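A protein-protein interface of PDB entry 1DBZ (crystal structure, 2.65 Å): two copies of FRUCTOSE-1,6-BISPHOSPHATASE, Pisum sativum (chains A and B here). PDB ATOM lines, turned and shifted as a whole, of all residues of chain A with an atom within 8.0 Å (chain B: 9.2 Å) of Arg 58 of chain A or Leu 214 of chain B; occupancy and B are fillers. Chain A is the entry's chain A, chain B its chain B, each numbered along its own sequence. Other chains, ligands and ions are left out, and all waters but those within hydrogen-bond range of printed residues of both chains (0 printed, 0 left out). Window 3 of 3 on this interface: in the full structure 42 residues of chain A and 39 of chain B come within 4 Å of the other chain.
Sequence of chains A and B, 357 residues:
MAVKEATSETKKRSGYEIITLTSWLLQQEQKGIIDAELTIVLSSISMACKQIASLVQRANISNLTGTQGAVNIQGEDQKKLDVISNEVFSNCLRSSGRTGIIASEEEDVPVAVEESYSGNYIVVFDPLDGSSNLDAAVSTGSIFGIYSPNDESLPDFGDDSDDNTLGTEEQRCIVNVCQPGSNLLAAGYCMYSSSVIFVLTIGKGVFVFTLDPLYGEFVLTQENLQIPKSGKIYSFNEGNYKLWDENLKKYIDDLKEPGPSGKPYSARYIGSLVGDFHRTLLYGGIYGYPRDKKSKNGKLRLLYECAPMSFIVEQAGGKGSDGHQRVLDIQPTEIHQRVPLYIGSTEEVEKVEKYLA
The side-chain hydroxyl of Ser 62 of chain A is in hydrogen-bond range of the backbone carbonyl oxygen of Arg 58 of chain A (3.0 Å).
O of Thr 210 of chain B is in hydrogen-bond range of N of Val 219 of chain B, at 2.6 Å.
OG1 of Thr 221 of chain B sits at hydrogen-bond distance from OG1 of Thr 210 of chain B (2.9 Å).
The backbone NH of Leu 214 of chain B lies within hydrogen-bond range of the side-chain carboxylate of Asp 212 of chain B.
N of Asp 212 of chain B is in hydrogen-bond range of O of Glu 217 of chain B (3.0 Å).
Of the printed residues of chain B, Gln 57 of chain A touches Ser 194 (3.5 Å), Ser 195 (3.7 Å) and Pro 213 (3.7 Å).
Of the printed residues of chain B, Arg 58 of chain A touches Asp 212 (2.8 Å), Pro 213 (3.1 Å) and Leu 214 (3.7 Å).
No residue of chain B comes within 4 Å of Ala 59 of chain A.
Asn 63 of chain A touches none of the printed residues of chain B.
Val 196 of chain B touches none of the printed residues of chain A.
Of the printed residues of chain A, Ile 197 of chain B touches Asn 60 (3.5 Å).
Of the printed residues of chain A, Thr 210 of chain B touches Asn 60 (2.9 Å).
Of chain A, only Gln 57 (3.7 Å) and Arg 58 (3.1 Å) come within 4 Å of Pro 213 of chain B.
Of chain A, only Arg 58 (3.7 Å) comes within 4 Å of Leu 214 of chain B.
Printed residues of chain A within 4 Å of Thr 221 of chain B: Asn 60 and Leu 64.
No position is printed for both chains.
Among the printed residues, merely in contact across the chains: Val 56 of chain A with Ser 194 of chain B, Gln 57 of chain A with Ser 194 of chain B, Gln 57 of chain A with Ser 195 of chain B, Gln 57 of chain A with Pro 213 of chain B, Arg 58 of chain A with Pro 213 of chain B, Arg 58 of chain A with Leu 214 of chain B, Asn 60 of chain A with Ser 195 of chain B, Asn 60 of chain A with Ile 197 of chain B, Asn 60 of chain A with Thr 221 of chain B, Ile 61 of chain A with Asp 212 of chain B and Leu 64 of chain A with Thr 221 of chain B.
Of the 15 printed residues of chain B, 8 touch a printed residue of chain A.
Along chain B the printed residues that touch a printed residue of chain A span positions 194 to 221.
The side-chain carboxylate (OD1) of Asp 212 of chain B is in salt-bridge range of the guanidinium group (NE) of Arg 58 of chain A (2.8 Å).
ND2 of Asn 60 of chain A sits at hydrogen-bond distance from OG1 of Thr 210 of chain B, at 2.9 Å.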
ATOM      1  N   ILE A  52      12.152   4.281  14.356  1.00  0.00           N
ATOM      2  CA  ILE A  52      13.394   3.812  13.772  1.00  0.00           C
ATOM      3  C   ILE A  52      14.526   4.302  14.657  1.00  0.00           C
ATOM      4  O   ILE A  52      15.474   3.576  14.921  1.00  0.00           O
ATOM      5  CB  ILE A  52      13.567   4.337  12.336  1.00  0.00           C
ATOM      6  CG1 ILE A  52      12.403   3.850  11.460  1.00  0.00           C
ATOM      7  CG2 ILE A  52      14.910   3.879  11.771  1.00  0.00           C
ATOM      8  CD1 ILE A  52      12.467   4.295  10.001  1.00  0.00           C
ATOM      9  N   ALA A  53      14.372   5.509  15.175  1.00  0.00           N
ATOM     10  CA  ALA A  53      15.370   6.081  16.048  1.00  0.00           C
ATOM     11  C   ALA A  53      15.577   5.180  17.252  1.00  0.00           C
ATOM     12  O   ALA A  53      16.699   5.009  17.729  1.00  0.00           O
ATOM     13  CB  ALA A  53      14.936   7.446  16.498  1.00  0.00           C
ATOM     14  N   SER A  54      14.497   4.570  17.720  1.00  0.00           N
ATOM     15  CA  SER A  54      14.569   3.683  18.878  1.00  0.00           C
ATOM     16  C   SER A  54      15.159   2.308  18.538  1.00  0.00           C
ATOM     17  O   SER A  54      15.777   1.661  19.385  1.00  0.00           O
ATOM     18  CB  SER A  54      13.174   3.527  19.495  1.00  0.00           C
ATOM     19  OG  SER A  54      13.244   3.065  20.832  1.00  0.00           O
ATOM     20  N   LEU A  55      14.943   1.856  17.306  1.00  0.00           N
ATOM     21  CA  LEU A  55      15.463   0.576  16.871  1.00  0.00           C
ATOM     22  C   LEU A  55      16.972   0.663  16.829  1.00  0.00           C
ATOM     23  O   LEU A  55      17.682  -0.250  17.251  1.00  0.00           O
ATOM     24  CB  LEU A  55      14.941   0.251  15.479  1.00  0.00           C
ATOM     25  CG  LEU A  55      13.432   0.063  15.380  1.00  0.00           C
ATOM     26  CD1 LEU A  55      13.018  -0.249  13.945  1.00  0.00           C
ATOM     27  CD2 LEU A  55      13.025  -1.059  16.300  1.00  0.00           C
ATOM     28  N   VAL A  56      17.450   1.791  16.321  1.00  0.00           N
ATOM     29  CA  VAL A  56      18.868   2.052  16.191  1.00  0.00           C
ATOM     30  C   VAL A  56      19.565   2.083  17.551  1.00  0.00           C
ATOM     31  O   VAL A  56      20.609   1.471  17.742  1.00  0.00           O
ATOM     32  CB  VAL A  56      19.094   3.377  15.449  1.00  0.00           C
ATOM     33  CG1 VAL A  56      20.537   3.777  15.527  1.00  0.00           C
ATOM     34  CG2 VAL A  56      18.675   3.245  13.999  1.00  0.00           C
ATOM     35  N   GLN A  57      18.948   2.756  18.506  1.00  0.00           N
ATOM     36  CA  GLN A  57      19.509   2.876  19.838  1.00  0.00           C
ATOM     37  C   GLN A  57      19.641   1.584  20.642  1.00  0.00           C
ATOM     38  O   GLN A  57      20.583   1.441  21.436  1.00  0.00           O
ATOM     39  CB  GLN A  57      18.699   3.889  20.622  1.00  0.00           C
ATOM     40  CG  GLN A  57      18.627   5.220  19.917  1.00  0.00           C
ATOM     41  CD  GLN A  57      17.722   6.230  20.596  1.00  0.00           C
ATOM     42  OE1 GLN A  57      17.028   5.934  21.577  1.00  0.00           O
ATOM     43  NE2 GLN A  57      17.728   7.444  20.070  1.00  0.00           N
ATOM     44  N   ARG A  58      18.704   0.656  20.443  1.00  0.00           N
ATOM     45  CA  ARG A  58      18.687  -0.626  21.157  1.00  0.00           C
ATOM     46  C   ARG A  58      19.164  -1.799  20.325  1.00  0.00           C
ATOM     47  O   ARG A  58      19.126  -2.929  20.789  1.00  0.00           O
ATOM     48  CB  ARG A  58      17.287  -0.956  21.660  1.00  0.00           C
ATOM     49  CG  ARG A  58      16.669   0.115  22.511  1.00  0.00           C
ATOM     50  CD  ARG A  58      15.323  -0.312  23.078  1.00  0.00           C
ATOM     51  NE  ARG A  58      15.451  -1.365  24.087  1.00  0.00           N
ATOM     52  CZ  ARG A  58      15.033  -2.613  23.909  1.00  0.00           C
ATOM     53  NH1 ARG A  58      14.458  -2.965  22.757  1.00  0.00           N
ATOM     54  NH2 ARG A  58      15.193  -3.507  24.874  1.00  0.00           N
ATOM     55  N   ALA A  59      19.623  -1.540  19.109  1.00  0.00           N
ATOM     56  CA  ALA A  59      20.097  -2.603  18.235  1.00  0.00           C
ATOM     57  C   ALA A  59      21.006  -3.641  18.901  1.00  0.00           C
ATOM     58  O   ALA A  59      20.841  -4.828  18.675  1.00  0.00           O
ATOM     59  CB  ALA A  59      20.769  -2.009  17.039  1.00  0.00           C
ATOM     60  N   ASN A  60      21.957  -3.211  19.724  1.00  0.00           N
ATOM     61  CA  ASN A  60      22.854  -4.154  20.404  1.00  0.00           C
ATOM     62  C   ASN A  60      22.123  -5.120  21.322  1.00  0.00           C
ATOM     63  O   ASN A  60      22.415  -6.304  21.332  1.00  0.00           O
ATOM     64  CB  ASN A  60      23.880  -3.406  21.227  1.00  0.00           C
ATOM     65  CG  ASN A  60      24.733  -2.524  20.394  1.00  0.00           C
ATOM     66  OD1 ASN A  60      24.941  -2.778  19.212  1.00  0.00           O
ATOM     67  ND2 ASN A  60      25.239  -1.473  20.996  1.00  0.00           N
ATOM     68  N   ILE A  61      21.234  -4.580  22.145  1.00  0.00           N
ATOM     69  CA  ILE A  61      20.430  -5.358  23.070  1.00  0.00           C
ATOM     70  C   ILE A  61      19.481  -6.228  22.266  1.00  0.00           C
ATOM     71  O   ILE A  61      19.248  -7.384  22.604  1.00  0.00           O
ATOM     72  CB  ILE A  61      19.597  -4.442  23.942  1.00  0.00           C
ATOM     73  CG1 ILE A  61      20.513  -3.474  24.668  1.00  0.00           C
ATOM     74  CG2 ILE A  61      18.756  -5.247  24.908  1.00  0.00           C
ATOM     75  CD1 ILE A  61      19.790  -2.341  25.287  1.00  0.00           C
ATOM     76  N   SER A  62      18.923  -5.660  21.204  1.00  0.00           N
ATOM     77  CA  SER A  62      18.014  -6.382  20.330  1.00  0.00           C
ATOM     78  C   SER A  62      18.706  -7.634  19.792  1.00  0.00           C
ATOM     79  O   SER A  62      18.092  -8.699  19.693  1.00  0.00           O
ATOM     80  CB  SER A  62      17.583  -5.500  19.150  1.00  0.00           C
ATOM     81  OG  SER A  62      16.769  -4.411  19.553  1.00  0.00           O
ATOM     82  N   ASN A  63      19.994  -7.506  19.475  1.00  0.00           N
ATOM     83  CA  ASN A  63      20.763  -8.626  18.940  1.00  0.00           C
ATOM     84  C   ASN A  63      21.114  -9.710  19.957  1.00  0.00           C
ATOM     85  O   ASN A  63      21.465 -10.828  19.567  1.00  0.00           O
ATOM     86  CB  ASN A  63      22.003  -8.121  18.212  1.00  0.00           C
ATOM     87  CG  ASN A  63      21.652  -7.264  17.015  1.00  0.00           C
ATOM     88  OD1 ASN A  63      20.717  -7.568  16.272  1.00  0.00           O
ATOM     89  ND2 ASN A  63      22.377  -6.169  16.839  1.00  0.00           N
ATOM     90  N   LEU A  64      21.002  -9.383  21.251  1.00  0.00           N
ATOM     91  CA  LEU A  64      21.264 -10.339  22.341  1.00  0.00           C
ATOM     92  C   LEU A  64      20.065 -11.261  22.503  1.00  0.00           C
ATOM     93  O   LEU A  64      20.144 -12.295  23.168  1.00  0.00           O
ATOM     94  CB  LEU A  64      21.465  -9.638  23.683  1.00  0.00           C
ATOM     95  CG  LEU A  64      22.599  -8.647  23.880  1.00  0.00           C
ATOM     96  CD1 LEU A  64      22.817  -8.481  25.385  1.00  0.00           C
ATOM     97  CD2 LEU A  64      23.851  -9.153  23.178  1.00  0.00           C
ATOM     98  N   THR A  65      18.933 -10.813  21.969  1.00  0.00           N
ATOM     99  CA  THR A  65      17.687 -11.563  22.001  1.00  0.00           C
ATOM    100  C   THR A  65      17.325 -11.973  20.572  1.00  0.00           C
ATOM    101  O   THR A  65      16.678 -12.997  20.349  1.00  0.00           O
ATOM    102  CB  THR A  65      16.584 -10.707  22.601  1.00  0.00           C
ATOM    103  N   LEU A  81      18.032  -4.611   9.981  1.00  0.00           N
ATOM    104  CA  LEU A  81      17.521  -3.399  10.580  1.00  0.00           C
ATOM    105  C   LEU A  81      16.863  -2.607   9.470  1.00  0.00           C
ATOM    106  O   LEU A  81      15.889  -1.896   9.704  1.00  0.00           O
ATOM    107  CB  LEU A  81      18.664  -2.599  11.165  1.00  0.00           C
ATOM    108  CG  LEU A  81      18.207  -1.496  12.104  1.00  0.00           C
ATOM    109  CD1 LEU A  81      17.268  -2.057  13.170  1.00  0.00           C
ATOM    110  CD2 LEU A  81      19.438  -0.872  12.737  1.00  0.00           C
ATOM    111  N   ILE B  18      19.782 -11.339  30.978  1.00  0.00           N
ATOM    112  CA  ILE B  18      19.937  -9.906  31.005  1.00  0.00           C
ATOM    113  C   ILE B  18      20.884  -9.575  32.140  1.00  0.00           C
ATOM    114  O   ILE B  18      20.586  -9.813  33.319  1.00  0.00           O
ATOM    115  CB  ILE B  18      18.587  -9.178  31.216  1.00  0.00           C
ATOM    116  CG1 ILE B  18      17.701  -9.324  29.975  1.00  0.00           C
ATOM    117  CG2 ILE B  18      18.817  -7.706  31.468  1.00  0.00           C
ATOM    118  CD1 ILE B  18      16.305  -8.701  30.115  1.00  0.00           C
ATOM    119  N   SER B 194      24.741   7.442  17.885  1.00  0.00           N
ATOM    120  CA  SER B 194      23.441   6.887  17.505  1.00  0.00           C
ATOM    121  C   SER B 194      23.017   5.874  18.573  1.00  0.00           C
ATOM    122  O   SER B 194      21.875   5.441  18.629  1.00  0.00           O
ATOM    123  CB  SER B 194      23.508   6.207  16.130  1.00  0.00           C
ATOM    124  OG  SER B 194      24.111   4.933  16.205  1.00  0.00           O
ATOM    125  N   SER B 195      23.943   5.586  19.475  1.00  0.00           N
ATOM    126  CA  SER B 195      23.755   4.647  20.553  1.00  0.00           C
ATOM    127  C   SER B 195      24.623   5.146  21.699  1.00  0.00           C
ATOM    128  O   SER B 195      25.587   5.866  21.460  1.00  0.00           O
ATOM    129  CB  SER B 195      24.266   3.300  20.084  1.00  0.00           C
ATOM    130  OG  SER B 195      24.110   2.344  21.097  1.00  0.00           O
ATOM    131  N   VAL B 196      24.282   4.814  22.938  1.00  0.00           N
ATOM    132  CA  VAL B 196      25.095   5.243  24.064  1.00  0.00           C
ATOM    133  C   VAL B 196      25.785   4.021  24.613  1.00  0.00           C
ATOM    134  O   VAL B 196      25.132   3.144  25.155  1.00  0.00           O
ATOM    135  CB  VAL B 196      24.247   5.898  25.138  1.00  0.00           C
ATOM    136  CG1 VAL B 196      25.109   6.259  26.320  1.00  0.00           C
ATOM    137  CG2 VAL B 196      23.600   7.140  24.592  1.00  0.00           C
ATOM    138  N   ILE B 197      27.103   3.949  24.427  1.00  0.00           N
ATOM    139  CA  ILE B 197      27.918   2.809  24.875  1.00  0.00           C
ATOM    140  C   ILE B 197      28.812   3.134  26.053  1.00  0.00           C
ATOM    141  O   ILE B 197      29.419   4.181  26.107  1.00  0.00           O
ATOM    142  CB  ILE B 197      28.827   2.303  23.740  1.00  0.00           C
ATOM    143  CG1 ILE B 197      28.018   2.062  22.485  1.00  0.00           C
ATOM    144  CG2 ILE B 197      29.455   1.009  24.120  1.00  0.00           C
ATOM    145  CD1 ILE B 197      26.872   1.153  22.720  1.00  0.00           C
ATOM    146  N   THR B 210      25.548  -1.579  26.592  1.00  0.00           N
ATOM    147  CA  THR B 210      24.680  -0.686  25.829  1.00  0.00           C
ATOM    148  C   THR B 210      23.583  -0.146  26.740  1.00  0.00           C
ATOM    149  O   THR B 210      23.057  -0.871  27.574  1.00  0.00           O
ATOM    150  CB  THR B 210      24.012  -1.412  24.649  1.00  0.00           C
ATOM    151  OG1 THR B 210      25.009  -2.034  23.837  1.00  0.00           O
ATOM    152  CG2 THR B 210      23.245  -0.439  23.803  1.00  0.00           C
ATOM    153  N   LEU B 211      23.246   1.128  26.585  1.00  0.00           N
ATOM    154  CA  LEU B 211      22.192   1.758  27.383  1.00  0.00           C
ATOM    155  C   LEU B 211      20.835   1.486  26.770  1.00  0.00           C
ATOM    156  O   LEU B 211      20.621   1.831  25.612  1.00  0.00           O
ATOM    157  CB  LEU B 211      22.375   3.263  27.387  1.00  0.00           C
ATOM    158  CG  LEU B 211      21.212   4.015  28.004  1.00  0.00           C
ATOM    159  CD1 LEU B 211      21.360   3.941  29.498  1.00  0.00           C
ATOM    160  CD2 LEU B 211      21.221   5.457  27.541  1.00  0.00           C
ATOM    161  N   ASP B 212      19.933   0.867  27.530  1.00  0.00           N
ATOM    162  CA  ASP B 212      18.586   0.600  27.037  1.00  0.00           C
ATOM    163  C   ASP B 212      17.773   1.854  27.294  1.00  0.00           C
ATOM    164  O   ASP B 212      17.585   2.261  28.434  1.00  0.00           O
ATOM    165  CB  ASP B 212      17.943  -0.566  27.771  1.00  0.00           C
ATOM    166  CG  ASP B 212      16.657  -1.022  27.115  1.00  0.00           C
ATOM    167  OD1 ASP B 212      15.892  -0.186  26.592  1.00  0.00           O
ATOM    168  OD2 ASP B 212      16.412  -2.239  27.120  1.00  0.00           O
ATOM    169  N   PRO B 213      17.288   2.486  26.227  1.00  0.00           N
ATOM    170  CA  PRO B 213      16.488   3.708  26.273  1.00  0.00           C
ATOM    171  C   PRO B 213      15.244   3.542  27.131  1.00  0.00           C
ATOM    172  O   PRO B 213      14.935   4.388  27.972  1.00  0.00           O
ATOM    173  CB  PRO B 213      16.097   3.898  24.810  1.00  0.00           C
ATOM    174  CG  PRO B 213      17.228   3.289  24.087  1.00  0.00           C
ATOM    175  CD  PRO B 213      17.474   2.036  24.845  1.00  0.00           C
ATOM    176  N   LEU B 214      14.565   2.419  26.934  1.00  0.00           N
ATOM    177  CA  LEU B 214      13.336   2.117  27.642  1.00  0.00           C
ATOM    178  C   LEU B 214      13.443   2.052  29.163  1.00  0.00           C
ATOM    179  O   LEU B 214      12.703   2.736  29.871  1.00  0.00           O
ATOM    180  CB  LEU B 214      12.750   0.810  27.106  1.00  0.00           C
ATOM    181  CG  LEU B 214      12.706   0.648  25.579  1.00  0.00           C
ATOM    182  CD1 LEU B 214      11.972  -0.640  25.188  1.00  0.00           C
ATOM    183  CD2 LEU B 214      12.027   1.852  24.956  1.00  0.00           C
ATOM    184  N   TYR B 215      14.389   1.259  29.661  1.00  0.00           N
ATOM    185  CA  TYR B 215      14.564   1.065  31.098  1.00  0.00           C
ATOM    186  C   TYR B 215      15.660   1.862  31.760  1.00  0.00           C
ATOM    187  O   TYR B 215      15.866   1.743  32.962  1.00  0.00           O
ATOM    188  CB  TYR B 215      14.735  -0.421  31.377  1.00  0.00           C
ATOM    189  CG  TYR B 215      13.707  -1.186  30.605  1.00  0.00           C
ATOM    190  CD1 TYR B 215      14.075  -2.172  29.700  1.00  0.00           C
ATOM    191  CD2 TYR B 215      12.362  -0.831  30.686  1.00  0.00           C
ATOM    192  CE1 TYR B 215      13.116  -2.785  28.877  1.00  0.00           C
ATOM    193  CE2 TYR B 215      11.402  -1.430  29.881  1.00  0.00           C
ATOM    194  CZ  TYR B 215      11.777  -2.405  28.975  1.00  0.00           C
ATOM    195  OH  TYR B 215      10.814  -2.994  28.182  1.00  0.00           O
ATOM    196  N   GLY B 216      16.340   2.696  30.985  1.00  0.00           N
ATOM    197  CA  GLY B 216      17.404   3.511  31.543  1.00  0.00           C
ATOM    198  C   GLY B 216      18.482   2.731  32.279  1.00  0.00           C
ATOM    199  O   GLY B 216      18.971   3.186  33.315  1.00  0.00           O
ATOM    200  N   GLU B 217      18.842   1.559  31.758  1.00  0.00           N
ATOM    201  CA  GLU B 217      19.874   0.722  32.369  1.00  0.00           C
ATOM    202  C   GLU B 217      20.864   0.154  31.350  1.00  0.00           C
ATOM    203  O   GLU B 217      20.470  -0.248  30.251  1.00  0.00           O
ATOM    204  CB  GLU B 217      19.239  -0.418  33.159  1.00  0.00           C
ATOM    205  CG  GLU B 217      18.474   0.063  34.370  1.00  0.00           C
ATOM    206  CD  GLU B 217      19.115  -0.332  35.683  1.00  0.00           C
ATOM    207  OE1 GLU B 217      20.262   0.081  35.985  1.00  0.00           O
ATOM    208  OE2 GLU B 217      18.441  -1.060  36.429  1.00  0.00           O
ATOM    209  N   VAL B 219      23.087  -2.450  29.654  1.00  0.00           N
ATOM    210  CA  VAL B 219      23.020  -3.887  29.473  1.00  0.00           C
ATOM    211  C   VAL B 219      24.282  -4.429  28.821  1.00  0.00           C
ATOM    212  O   VAL B 219      24.630  -3.990  27.733  1.00  0.00           O
ATOM    213  CB  VAL B 219      21.821  -4.241  28.561  1.00  0.00           C
ATOM    214  CG1 VAL B 219      21.710  -5.753  28.378  1.00  0.00           C
ATOM    215  CG2 VAL B 219      20.531  -3.635  29.114  1.00  0.00           C
ATOM    216  N   THR B 221      26.423  -6.040  26.510  1.00  0.00           N
ATOM    217  CA  THR B 221      26.242  -6.553  25.161  1.00  0.00           C
ATOM    218  C   THR B 221      27.486  -7.223  24.574  1.00  0.00           C
ATOM    219  O   THR B 221      27.429  -7.777  23.477  1.00  0.00           O
ATOM    220  CB  THR B 221      25.772  -5.457  24.214  1.00  0.00           C
ATOM    221  OG1 THR B 221      26.705  -4.379  24.242  1.00  0.00           O
ATOM    222  CG2 THR B 221      24.415  -4.942  24.640  1.00  0.00           C
